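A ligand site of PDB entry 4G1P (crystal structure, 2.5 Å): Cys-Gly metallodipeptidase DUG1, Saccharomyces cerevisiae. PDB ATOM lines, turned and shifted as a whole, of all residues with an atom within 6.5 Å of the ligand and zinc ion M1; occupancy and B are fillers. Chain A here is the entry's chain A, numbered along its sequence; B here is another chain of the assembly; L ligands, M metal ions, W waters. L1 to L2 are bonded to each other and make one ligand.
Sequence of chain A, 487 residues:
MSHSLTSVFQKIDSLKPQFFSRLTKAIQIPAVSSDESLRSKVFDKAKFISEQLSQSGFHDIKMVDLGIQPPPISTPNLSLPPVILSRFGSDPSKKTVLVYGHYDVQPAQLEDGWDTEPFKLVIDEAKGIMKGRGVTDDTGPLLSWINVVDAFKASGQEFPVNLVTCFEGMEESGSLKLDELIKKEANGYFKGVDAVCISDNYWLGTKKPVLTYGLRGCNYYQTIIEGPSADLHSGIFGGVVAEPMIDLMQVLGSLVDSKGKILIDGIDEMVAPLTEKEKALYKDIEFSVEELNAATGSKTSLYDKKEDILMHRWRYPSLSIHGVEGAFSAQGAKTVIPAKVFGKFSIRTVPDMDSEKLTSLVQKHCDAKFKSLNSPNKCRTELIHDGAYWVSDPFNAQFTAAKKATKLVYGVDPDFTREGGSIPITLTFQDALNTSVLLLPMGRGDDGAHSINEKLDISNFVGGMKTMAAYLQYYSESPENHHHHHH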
ATOM      1  N   HIS A 102      -6.367  -1.260 -11.335  1.00  0.00           N
ATOM      2  CA  HIS A 102      -7.693  -1.684 -10.911  1.00  0.00           C
ATOM      3  C   HIS A 102      -8.681  -0.562 -10.857  1.00  0.00           C
ATOM      4  O   HIS A 102      -8.366   0.555 -10.408  1.00  0.00           O
ATOM      5  CB  HIS A 102      -7.641  -2.456  -9.585  1.00  0.00           C
ATOM      6  CG  HIS A 102      -7.275  -1.621  -8.394  1.00  0.00           C
ATOM      7  ND1 HIS A 102      -8.219  -0.953  -7.645  1.00  0.00           N
ATOM      8  CD2 HIS A 102      -6.088  -1.400  -7.781  1.00  0.00           C
ATOM      9  CE1 HIS A 102      -7.617  -0.333  -6.645  1.00  0.00           C
ATOM     10  NE2 HIS A 102      -6.325  -0.589  -6.701  1.00  0.00           N
ATOM     11  N   GLN A 106     -12.367   1.572  -2.772  1.00  0.00           N
ATOM     12  CA  GLN A 106     -12.859   1.475  -1.391  1.00  0.00           C
ATOM     13  C   GLN A 106     -14.196   2.213  -1.208  1.00  0.00           C
ATOM     14  O   GLN A 106     -14.476   3.166  -1.908  1.00  0.00           O
ATOM     15  CB  GLN A 106     -11.813   2.054  -0.433  1.00  0.00           C
ATOM     16  CG  GLN A 106     -10.591   1.180  -0.254  1.00  0.00           C
ATOM     17  CD  GLN A 106     -10.874  -0.034   0.596  1.00  0.00           C
ATOM     18  OE1 GLN A 106     -11.435   0.082   1.682  1.00  0.00           O
ATOM     19  NE2 GLN A 106     -10.503  -1.226   0.098  1.00  0.00           N
ATOM     20  N   ASP A 137      -6.029   5.619  -5.898  1.00  0.00           N
ATOM     21  CA  ASP A 137      -6.071   4.184  -5.693  1.00  0.00           C
ATOM     22  C   ASP A 137      -7.385   3.671  -6.265  1.00  0.00           C
ATOM     23  O   ASP A 137      -8.349   3.523  -5.509  1.00  0.00           O
ATOM     24  CB  ASP A 137      -5.969   3.894  -4.183  1.00  0.00           C
ATOM     25  CG  ASP A 137      -6.026   2.412  -3.853  1.00  0.00           C
ATOM     26  OD1 ASP A 137      -5.902   1.569  -4.763  1.00  0.00           O
ATOM     27  OD2 ASP A 137      -6.166   2.072  -2.658  1.00  0.00           O
ATOM     28  N   ASP A 138      -7.432   3.381  -7.563  1.00  0.00           N
ATOM     29  CA  ASP A 138      -6.294   3.337  -8.469  1.00  0.00           C
ATOM     30  C   ASP A 138      -6.687   3.931  -9.821  1.00  0.00           C
ATOM     31  O   ASP A 138      -6.050   3.670 -10.831  1.00  0.00           O
ATOM     32  CB  ASP A 138      -5.863   1.867  -8.661  1.00  0.00           C
ATOM     33  CG  ASP A 138      -4.569   1.696  -9.476  1.00  0.00           C
ATOM     34  OD1 ASP A 138      -3.592   2.451  -9.266  1.00  0.00           O
ATOM     35  OD2 ASP A 138      -4.528   0.789 -10.337  1.00  0.00           O
ATOM     36  N   GLU A 171      -9.802  -5.599  -6.917  1.00  0.00           N
ATOM     37  CA  GLU A 171      -8.563  -5.440  -6.167  1.00  0.00           C
ATOM     38  C   GLU A 171      -8.816  -5.119  -4.700  1.00  0.00           C
ATOM     39  O   GLU A 171      -8.108  -5.602  -3.822  1.00  0.00           O
ATOM     40  CB  GLU A 171      -7.648  -4.391  -6.784  1.00  0.00           C
ATOM     41  CG  GLU A 171      -6.171  -4.537  -6.444  1.00  0.00           C
ATOM     42  CD  GLU A 171      -5.730  -3.703  -5.246  1.00  0.00           C
ATOM     43  OE1 GLU A 171      -6.578  -3.065  -4.590  1.00  0.00           O
ATOM     44  OE2 GLU A 171      -4.505  -3.694  -4.950  1.00  0.00           O
ATOM     45  N   GLU A 172      -9.850  -4.327  -4.433  1.00  0.00           N
ATOM     46  CA  GLU A 172     -10.170  -3.944  -3.061  1.00  0.00           C
ATOM     47  C   GLU A 172     -10.974  -5.046  -2.360  1.00  0.00           C
ATOM     48  O   GLU A 172     -11.410  -4.874  -1.219  1.00  0.00           O
ATOM     49  CB  GLU A 172     -10.924  -2.610  -3.032  1.00  0.00           C
ATOM     50  CG  GLU A 172     -10.229  -1.449  -3.740  1.00  0.00           C
ATOM     51  CD  GLU A 172      -9.040  -0.902  -2.958  1.00  0.00           C
ATOM     52  OE1 GLU A 172      -8.752  -1.412  -1.857  1.00  0.00           O
ATOM     53  OE2 GLU A 172      -8.390   0.049  -3.448  1.00  0.00           O
ATOM     54  N   SER A 173     -11.152  -6.165  -3.045  1.00  0.00           N
ATOM     55  CA  SER A 173     -11.952  -7.277  -2.534  1.00  0.00           C
ATOM     56  C   SER A 173     -11.266  -8.628  -2.803  1.00  0.00           C
ATOM     57  O   SER A 173     -11.910  -9.595  -3.216  1.00  0.00           O
ATOM     58  CB  SER A 173     -13.348  -7.248  -3.160  1.00  0.00           C
ATOM     59  OG  SER A 173     -13.979  -5.993  -2.965  1.00  0.00           O
ATOM     60  N   GLY A 174      -9.953  -8.663  -2.596  1.00  0.00           N
ATOM     61  CA  GLY A 174      -9.197  -9.899  -2.711  1.00  0.00           C
ATOM     62  C   GLY A 174      -8.700 -10.303  -4.087  1.00  0.00           C
ATOM     63  O   GLY A 174      -8.077 -11.359  -4.218  1.00  0.00           O
ATOM     64  N   ASP A 200       0.406   1.405  -8.867  1.00  0.00           N
ATOM     65  CA  ASP A 200      -0.623   1.138  -7.872  1.00  0.00           C
ATOM     66  C   ASP A 200      -0.076   1.293  -6.466  1.00  0.00           C
ATOM     67  O   ASP A 200      -0.462   0.556  -5.552  1.00  0.00           O
ATOM     68  CB  ASP A 200      -1.148  -0.282  -8.059  1.00  0.00           C
ATOM     69  CG  ASP A 200      -2.594  -0.437  -7.622  1.00  0.00           C
ATOM     70  OD1 ASP A 200      -3.191   0.538  -7.118  1.00  0.00           O
ATOM     71  OD2 ASP A 200      -3.143  -1.541  -7.773  1.00  0.00           O
ATOM     72  N   TYR A 202       2.589   4.447  -4.048  1.00  0.00           N
ATOM     73  CA  TYR A 202       2.849   5.872  -3.808  1.00  0.00           C
ATOM     74  C   TYR A 202       4.303   6.092  -3.484  1.00  0.00           C
ATOM     75  O   TYR A 202       5.005   5.151  -3.110  1.00  0.00           O
ATOM     76  CB  TYR A 202       2.002   6.374  -2.636  1.00  0.00           C
ATOM     77  CG  TYR A 202       0.698   5.622  -2.578  1.00  0.00           C
ATOM     78  CD1 TYR A 202       0.590   4.435  -1.859  1.00  0.00           C
ATOM     79  CD2 TYR A 202      -0.401   6.054  -3.311  1.00  0.00           C
ATOM     80  CE1 TYR A 202      -0.590   3.706  -1.855  1.00  0.00           C
ATOM     81  CE2 TYR A 202      -1.577   5.346  -3.299  1.00  0.00           C
ATOM     82  CZ  TYR A 202      -1.680   4.179  -2.572  1.00  0.00           C
ATOM     83  OH  TYR A 202      -2.865   3.458  -2.572  1.00  0.00           O
ATOM     84  N   CYS A 218      -0.388  -9.834   2.338  1.00  0.00           N
ATOM     85  CA  CYS A 218      -1.448  -9.546   3.291  1.00  0.00           C
ATOM     86  C   CYS A 218      -2.344 -10.768   3.517  1.00  0.00           C
ATOM     87  O   CYS A 218      -2.886 -11.360   2.572  1.00  0.00           O
ATOM     88  CB  CYS A 218      -2.269  -8.331   2.841  1.00  0.00           C
ATOM     89  SG  CYS A 218      -3.489  -7.769   4.077  1.00  0.00           S
ATOM     90  N   ASN A 219      -2.475 -11.160   4.773  1.00  0.00           N
ATOM     91  CA  ASN A 219      -3.398 -12.231   5.142  1.00  0.00           C
ATOM     92  C   ASN A 219      -4.509 -11.645   6.008  1.00  0.00           C
ATOM     93  O   ASN A 219      -4.243 -11.080   7.080  1.00  0.00           O
ATOM     94  CB  ASN A 219      -2.666 -13.370   5.861  1.00  0.00           C
ATOM     95  CG  ASN A 219      -1.926 -14.280   4.899  1.00  0.00           C
ATOM     96  OD1 ASN A 219      -1.534 -13.868   3.810  1.00  0.00           O
ATOM     97  ND2 ASN A 219      -1.732 -15.528   5.299  1.00  0.00           N
ATOM     98  N   TYR A 220      -5.734 -11.736   5.536  1.00  0.00           N
ATOM     99  CA  TYR A 220      -6.826 -11.101   6.253  1.00  0.00           C
ATOM    100  C   TYR A 220      -7.686 -12.153   6.945  1.00  0.00           C
ATOM    101  O   TYR A 220      -8.206 -13.070   6.287  1.00  0.00           O
ATOM    102  CB  TYR A 220      -7.675 -10.251   5.304  1.00  0.00           C
ATOM    103  CG  TYR A 220      -8.436  -9.138   5.991  1.00  0.00           C
ATOM    104  CD1 TYR A 220      -9.557  -9.409   6.750  1.00  0.00           C
ATOM    105  CD2 TYR A 220      -8.021  -7.820   5.878  1.00  0.00           C
ATOM    106  CE1 TYR A 220     -10.252  -8.396   7.390  1.00  0.00           C
ATOM    107  CE2 TYR A 220      -8.711  -6.804   6.494  1.00  0.00           C
ATOM    108  CZ  TYR A 220      -9.827  -7.096   7.256  1.00  0.00           C
ATOM    109  OH  TYR A 220     -10.541  -6.095   7.874  1.00  0.00           O
ATOM    110  N   ARG A 348       0.531  -8.246   7.647  1.00  0.00           N
ATOM    111  CA  ARG A 348       1.358  -7.930   6.498  1.00  0.00           C
ATOM    112  C   ARG A 348       2.537  -8.888   6.453  1.00  0.00           C
ATOM    113  O   ARG A 348       3.341  -8.926   7.369  1.00  0.00           O
ATOM    114  CB  ARG A 348       1.833  -6.479   6.560  1.00  0.00           C
ATOM    115  CG  ARG A 348       0.704  -5.451   6.461  1.00  0.00           C
ATOM    116  CD  ARG A 348       0.088  -5.395   5.070  1.00  0.00           C
ATOM    117  NE  ARG A 348      -1.129  -4.597   5.080  1.00  0.00           N
ATOM    118  CZ  ARG A 348      -1.831  -4.262   3.991  1.00  0.00           C
ATOM    119  NH1 ARG A 348      -1.430  -4.617   2.771  1.00  0.00           N
ATOM    120  NH2 ARG A 348      -2.942  -3.533   4.136  1.00  0.00           N
ATOM    121  N   HIS A 385      -8.911 -13.470   2.903  1.00  0.00           N
ATOM    122  CA  HIS A 385      -8.112 -13.472   1.678  1.00  0.00           C
ATOM    123  C   HIS A 385      -6.621 -13.412   1.975  1.00  0.00           C
ATOM    124  O   HIS A 385      -6.201 -12.938   3.037  1.00  0.00           O
ATOM    125  CB  HIS A 385      -8.545 -12.368   0.714  1.00  0.00           C
ATOM    126  CG  HIS A 385      -8.184 -10.985   1.147  1.00  0.00           C
ATOM    127  ND1 HIS A 385      -9.129  -9.993   1.318  1.00  0.00           N
ATOM    128  CD2 HIS A 385      -6.986 -10.400   1.409  1.00  0.00           C
ATOM    129  CE1 HIS A 385      -8.531  -8.871   1.689  1.00  0.00           C
ATOM    130  NE2 HIS A 385      -7.228  -9.093   1.754  1.00  0.00           N
ATOM    131  N   GLY A 420       4.981  -0.869   2.134  1.00  0.00           N
ATOM    132  CA  GLY A 420       4.224  -1.456   3.230  1.00  0.00           C
ATOM    133  C   GLY A 420       2.924  -2.056   2.720  1.00  0.00           C
ATOM    134  O   GLY A 420       2.422  -3.042   3.262  1.00  0.00           O
ATOM    135  N   GLY A 421       2.380  -1.461   1.665  1.00  0.00           N
ATOM    136  CA  GLY A 421       1.141  -1.936   1.077  1.00  0.00           C
ATOM    137  C   GLY A 421       1.341  -3.199   0.262  1.00  0.00           C
ATOM    138  O   GLY A 421       2.450  -3.738   0.232  1.00  0.00           O
ATOM    139  N   SER A 422       0.287  -3.631  -0.415  1.00  0.00           N
ATOM    140  CA  SER A 422       0.285  -4.893  -1.138  1.00  0.00           C
ATOM    141  C   SER A 422      -0.380  -4.794  -2.488  1.00  0.00           C
ATOM    142  O   SER A 422      -1.359  -4.075  -2.662  1.00  0.00           O
ATOM    143  CB  SER A 422      -0.452  -5.933  -0.326  1.00  0.00           C
ATOM    144  OG  SER A 422       0.084  -5.990   0.965  1.00  0.00           O
ATOM    145  N   ILE A 423       0.154  -5.512  -3.453  1.00  0.00           N
ATOM    146  CA  ILE A 423      -0.522  -5.674  -4.720  1.00  0.00           C
ATOM    147  C   ILE A 423      -0.469  -7.147  -5.056  1.00  0.00           C
ATOM    148  O   ILE A 423       0.391  -7.591  -5.775  1.00  0.00           O
ATOM    149  CB  ILE A 423       0.132  -4.877  -5.838  1.00  0.00           C
ATOM    150  CG1 ILE A 423       0.286  -3.413  -5.425  1.00  0.00           C
ATOM    151  CG2 ILE A 423      -0.681  -5.005  -7.099  1.00  0.00           C
ATOM    152  CD1 ILE A 423       1.193  -2.594  -6.337  1.00  0.00           C
ATOM    153  N   PRO A 424      -1.402  -7.910  -4.491  1.00  0.00           N
ATOM    154  CA  PRO A 424      -1.472  -9.377  -4.575  1.00  0.00           C
ATOM    155  C   PRO A 424      -0.969 -10.057  -5.866  1.00  0.00           C
ATOM    156  O   PRO A 424      -0.200 -10.990  -5.699  1.00  0.00           O
ATOM    157  CB  PRO A 424      -2.955  -9.640  -4.342  1.00  0.00           C
ATOM    158  CG  PRO A 424      -3.323  -8.590  -3.340  1.00  0.00           C
ATOM    159  CD  PRO A 424      -2.518  -7.365  -3.695  1.00  0.00           C
ATOM    160  N   ALA A 449      -5.162   7.188   0.615  1.00  0.00           N
ATOM    161  CA  ALA A 449      -5.822   5.981   0.135  1.00  0.00           C
ATOM    162  C   ALA A 449      -6.457   5.212   1.306  1.00  0.00           C
ATOM    163  O   ALA A 449      -5.872   5.128   2.392  1.00  0.00           O
ATOM    164  CB  ALA A 449      -4.853   5.092  -0.619  1.00  0.00           C
ATOM    165  N   HIS A 450      -7.665   4.702   1.074  1.00  0.00           N
ATOM    166  CA  HIS A 450      -8.435   3.951   2.072  1.00  0.00           C
ATOM    167  C   HIS A 450      -8.886   4.836   3.226  1.00  0.00           C
ATOM    168  O   HIS A 450      -9.262   4.341   4.290  1.00  0.00           O
ATOM    169  CB  HIS A 450      -7.643   2.752   2.610  1.00  0.00           C
ATOM    170  CG  HIS A 450      -7.338   1.721   1.572  1.00  0.00           C
ATOM    171  ND1 HIS A 450      -7.024   0.420   1.902  1.00  0.00           N
ATOM    172  CD2 HIS A 450      -7.290   1.789   0.223  1.00  0.00           C
ATOM    173  CE1 HIS A 450      -6.803  -0.273   0.793  1.00  0.00           C
ATOM    174  NE2 HIS A 450      -6.957   0.542  -0.237  1.00  0.00           N
ATOM    175  N   HIS B 233      -4.314   3.756   5.926  1.00  0.00           N
ATOM    176  CA  HIS B 233      -4.154   2.521   5.162  1.00  0.00           C
ATOM    177  C   HIS B 233      -3.325   1.576   6.030  1.00  0.00           C
ATOM    178  O   HIS B 233      -2.232   1.923   6.455  1.00  0.00           O
ATOM    179  CB  HIS B 233      -3.435   2.824   3.849  1.00  0.00           C
ATOM    180  CG  HIS B 233      -3.317   1.648   2.928  1.00  0.00           C
ATOM    181  ND1 HIS B 233      -2.553   0.544   3.242  1.00  0.00           N
ATOM    182  CD2 HIS B 233      -3.872   1.399   1.721  1.00  0.00           C
ATOM    183  CE1 HIS B 233      -2.636  -0.331   2.249  1.00  0.00           C
ATOM    184  NE2 HIS B 233      -3.433   0.159   1.319  1.00  0.00           N
ATOM    185  N   SER B 234      -3.856   0.397   6.319  1.00  0.00           N
ATOM    186  CA  SER B 234      -3.194  -0.425   7.321  1.00  0.00           C
ATOM    187  C   SER B 234      -1.894  -1.047   6.819  1.00  0.00           C
ATOM    188  O   SER B 234      -1.158  -1.625   7.610  1.00  0.00           O
ATOM    189  CB  SER B 234      -4.126  -1.505   7.901  1.00  0.00           C
ATOM    190  OG  SER B 234      -4.248  -2.595   7.013  1.00  0.00           O
ATOM    191  N   GLY B 235      -1.640  -0.904   5.511  1.00  0.00           N
ATOM    192  CA  GLY B 235      -0.443  -1.446   4.892  1.00  0.00           C
ATOM    193  C   GLY B 235       0.675  -0.426   4.849  1.00  0.00           C
ATOM    194  O   GLY B 235       1.819  -0.720   5.161  1.00  0.00           O
ATOM    195  N   THR B 335      -8.853  -3.019   5.007  1.00  0.00           N
ATOM    196  CA  THR B 335      -7.488  -2.858   5.493  1.00  0.00           C
ATOM    197  C   THR B 335      -7.307  -1.424   5.916  1.00  0.00           C
ATOM    198  O   THR B 335      -6.754  -0.608   5.168  1.00  0.00           O
ATOM    199  CB  THR B 335      -6.468  -3.172   4.419  1.00  0.00           C
ATOM    200  OG1 THR B 335      -6.920  -2.664   3.168  1.00  0.00           O
ATOM    201  CG2 THR B 335      -6.263  -4.659   4.290  1.00  0.00           C
HETATM  202  N1  LIG L   1      -4.395  -0.564  -1.353  1.00  0.00           N
HETATM  203  C1  LIG L   1      -5.086  -1.529  -2.188  1.00  0.00           C
HETATM  204  C2  LIG L   1      -4.963  -2.838  -1.458  1.00  0.00           C
HETATM  205  O1  LIG L   1      -4.194  -3.721  -1.850  1.00  0.00           O
HETATM  206  N1  LG2 L   2      -5.724  -2.952  -0.373  1.00  0.00           N
HETATM  207  C1  LG2 L   2      -5.525  -3.996   0.613  1.00  0.00           C
HETATM  208  C2  LG2 L   2      -4.196  -3.754   1.339  1.00  0.00           C
HETATM  209  O1  LG2 L   2      -3.148  -3.625   0.717  1.00  0.00           O
HETATM  210  C3  LG2 L   2      -5.573  -5.382  -0.044  1.00  0.00           C
HETATM  211  S1  LG2 L   2      -5.392  -6.725   1.085  1.00  0.00           S
HETATM  212 ZN    ZN M   1      -6.721   0.179  -2.219  1.00  0.00          ZN
HETATM  213 ZN    ZN M   2      -3.405   0.214  -4.411  1.00  0.00          ZN
HETATM  214  O   HOH W   1      -8.476  -6.674  -1.287  1.00  0.00           O
HETATM  215  O   HOH W   2      -3.833  -9.138   0.186  1.00  0.00           O
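An oxygen (O1) of LG2 L2 lies within hydrogen-bond range of the guanidinium group (NH1) of Arg 348 (2.9 Å).
A ring nitrogen (NE2) of His 233 of chain B lies close to a nitrogen (N1) of LIG L1 (2.9 Å).
A sulfur (S1) of LG2 L2 lies close to a ring nitrogen (NE2) of His 385 (3.1 Å).
The side-chain sulfur (SG) of Cys 218 lies close to a sulfur (S1) of LG2 L2 (3.7 Å).
The side-chain carboxylate (OD1) of Asp 137 is in hydrogen-bond range of a ring nitrogen (NE2) of His 102 (2.9 Å).
OG1 of Thr 335 of chain B sits at hydrogen-bond distance from ND1 of His 450 (3.3 Å).
The side-chain carboxylate (OE1) of Glu 172 is in hydrogen-bond range of the side-chain amide nitrogen (NE2) of Gln 106 (2.6 Å).
NH1 of Arg 348 is in hydrogen-bond range of OG of Ser 422.
The guanidinium group of Arg 348 is in hydrogen-bond range of the side-chain hydroxyl of Ser 234 of chain B, at 3.3 Å.
O of His 385 sits at hydrogen-bond distance from N of Tyr 220, 2.8 Å away.
The side-chain carboxylate (OE1) of Glu 171 lies within hydrogen-bond range of a ring nitrogen (NE2) of His 102, 3.3 Å away.
O of Thr 335 of chain B sits at hydrogen-bond distance from N of Ser 234 of chain B, at 3.3 Å.
O1 of LIG L1 lies close to OE2 of Glu 171, 3.1 Å away.
O of Ser 422 sits close to O1 of LIG L1, 3.0 Å away.
Thr 335 of chain B touches the ligand.
Hydrophobic or aromatic side chains that line the ligand: His 385, His 450 and His 233 of chain B.
Within 4 Å of the ligand: Asp 137, Glu 171, Glu 172, Cys 218, Arg 348, His 385, Ser 422, His 450, His 233 of chain B and Thr 335 of chain B.
OD2 of Asp 137 is bound to zinc ion M1 (2.0 Å).
Zinc ion M1 is bound by a ring nitrogen (NE2) of His 450 (2.0 Å).
OE2 of Glu 172 binds zinc ion M1 (2.1 Å).
Zinc ion M1 is bound by a nitrogen (N1) of LIG L1 (2.6 Å).
Zinc ion M1 has four donor atoms within binding distance.
Slightly farther from zinc ion M1 lies the side-chain carboxylate (OE1) of Glu 172 (2.6 Å).
Water W2 lies within hydrogen-bond range of a sulfur (S1) of LG2 L2 (3.0 Å) and the backbone carbonyl oxygen (O) of Cys 218 (3.4 Å).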
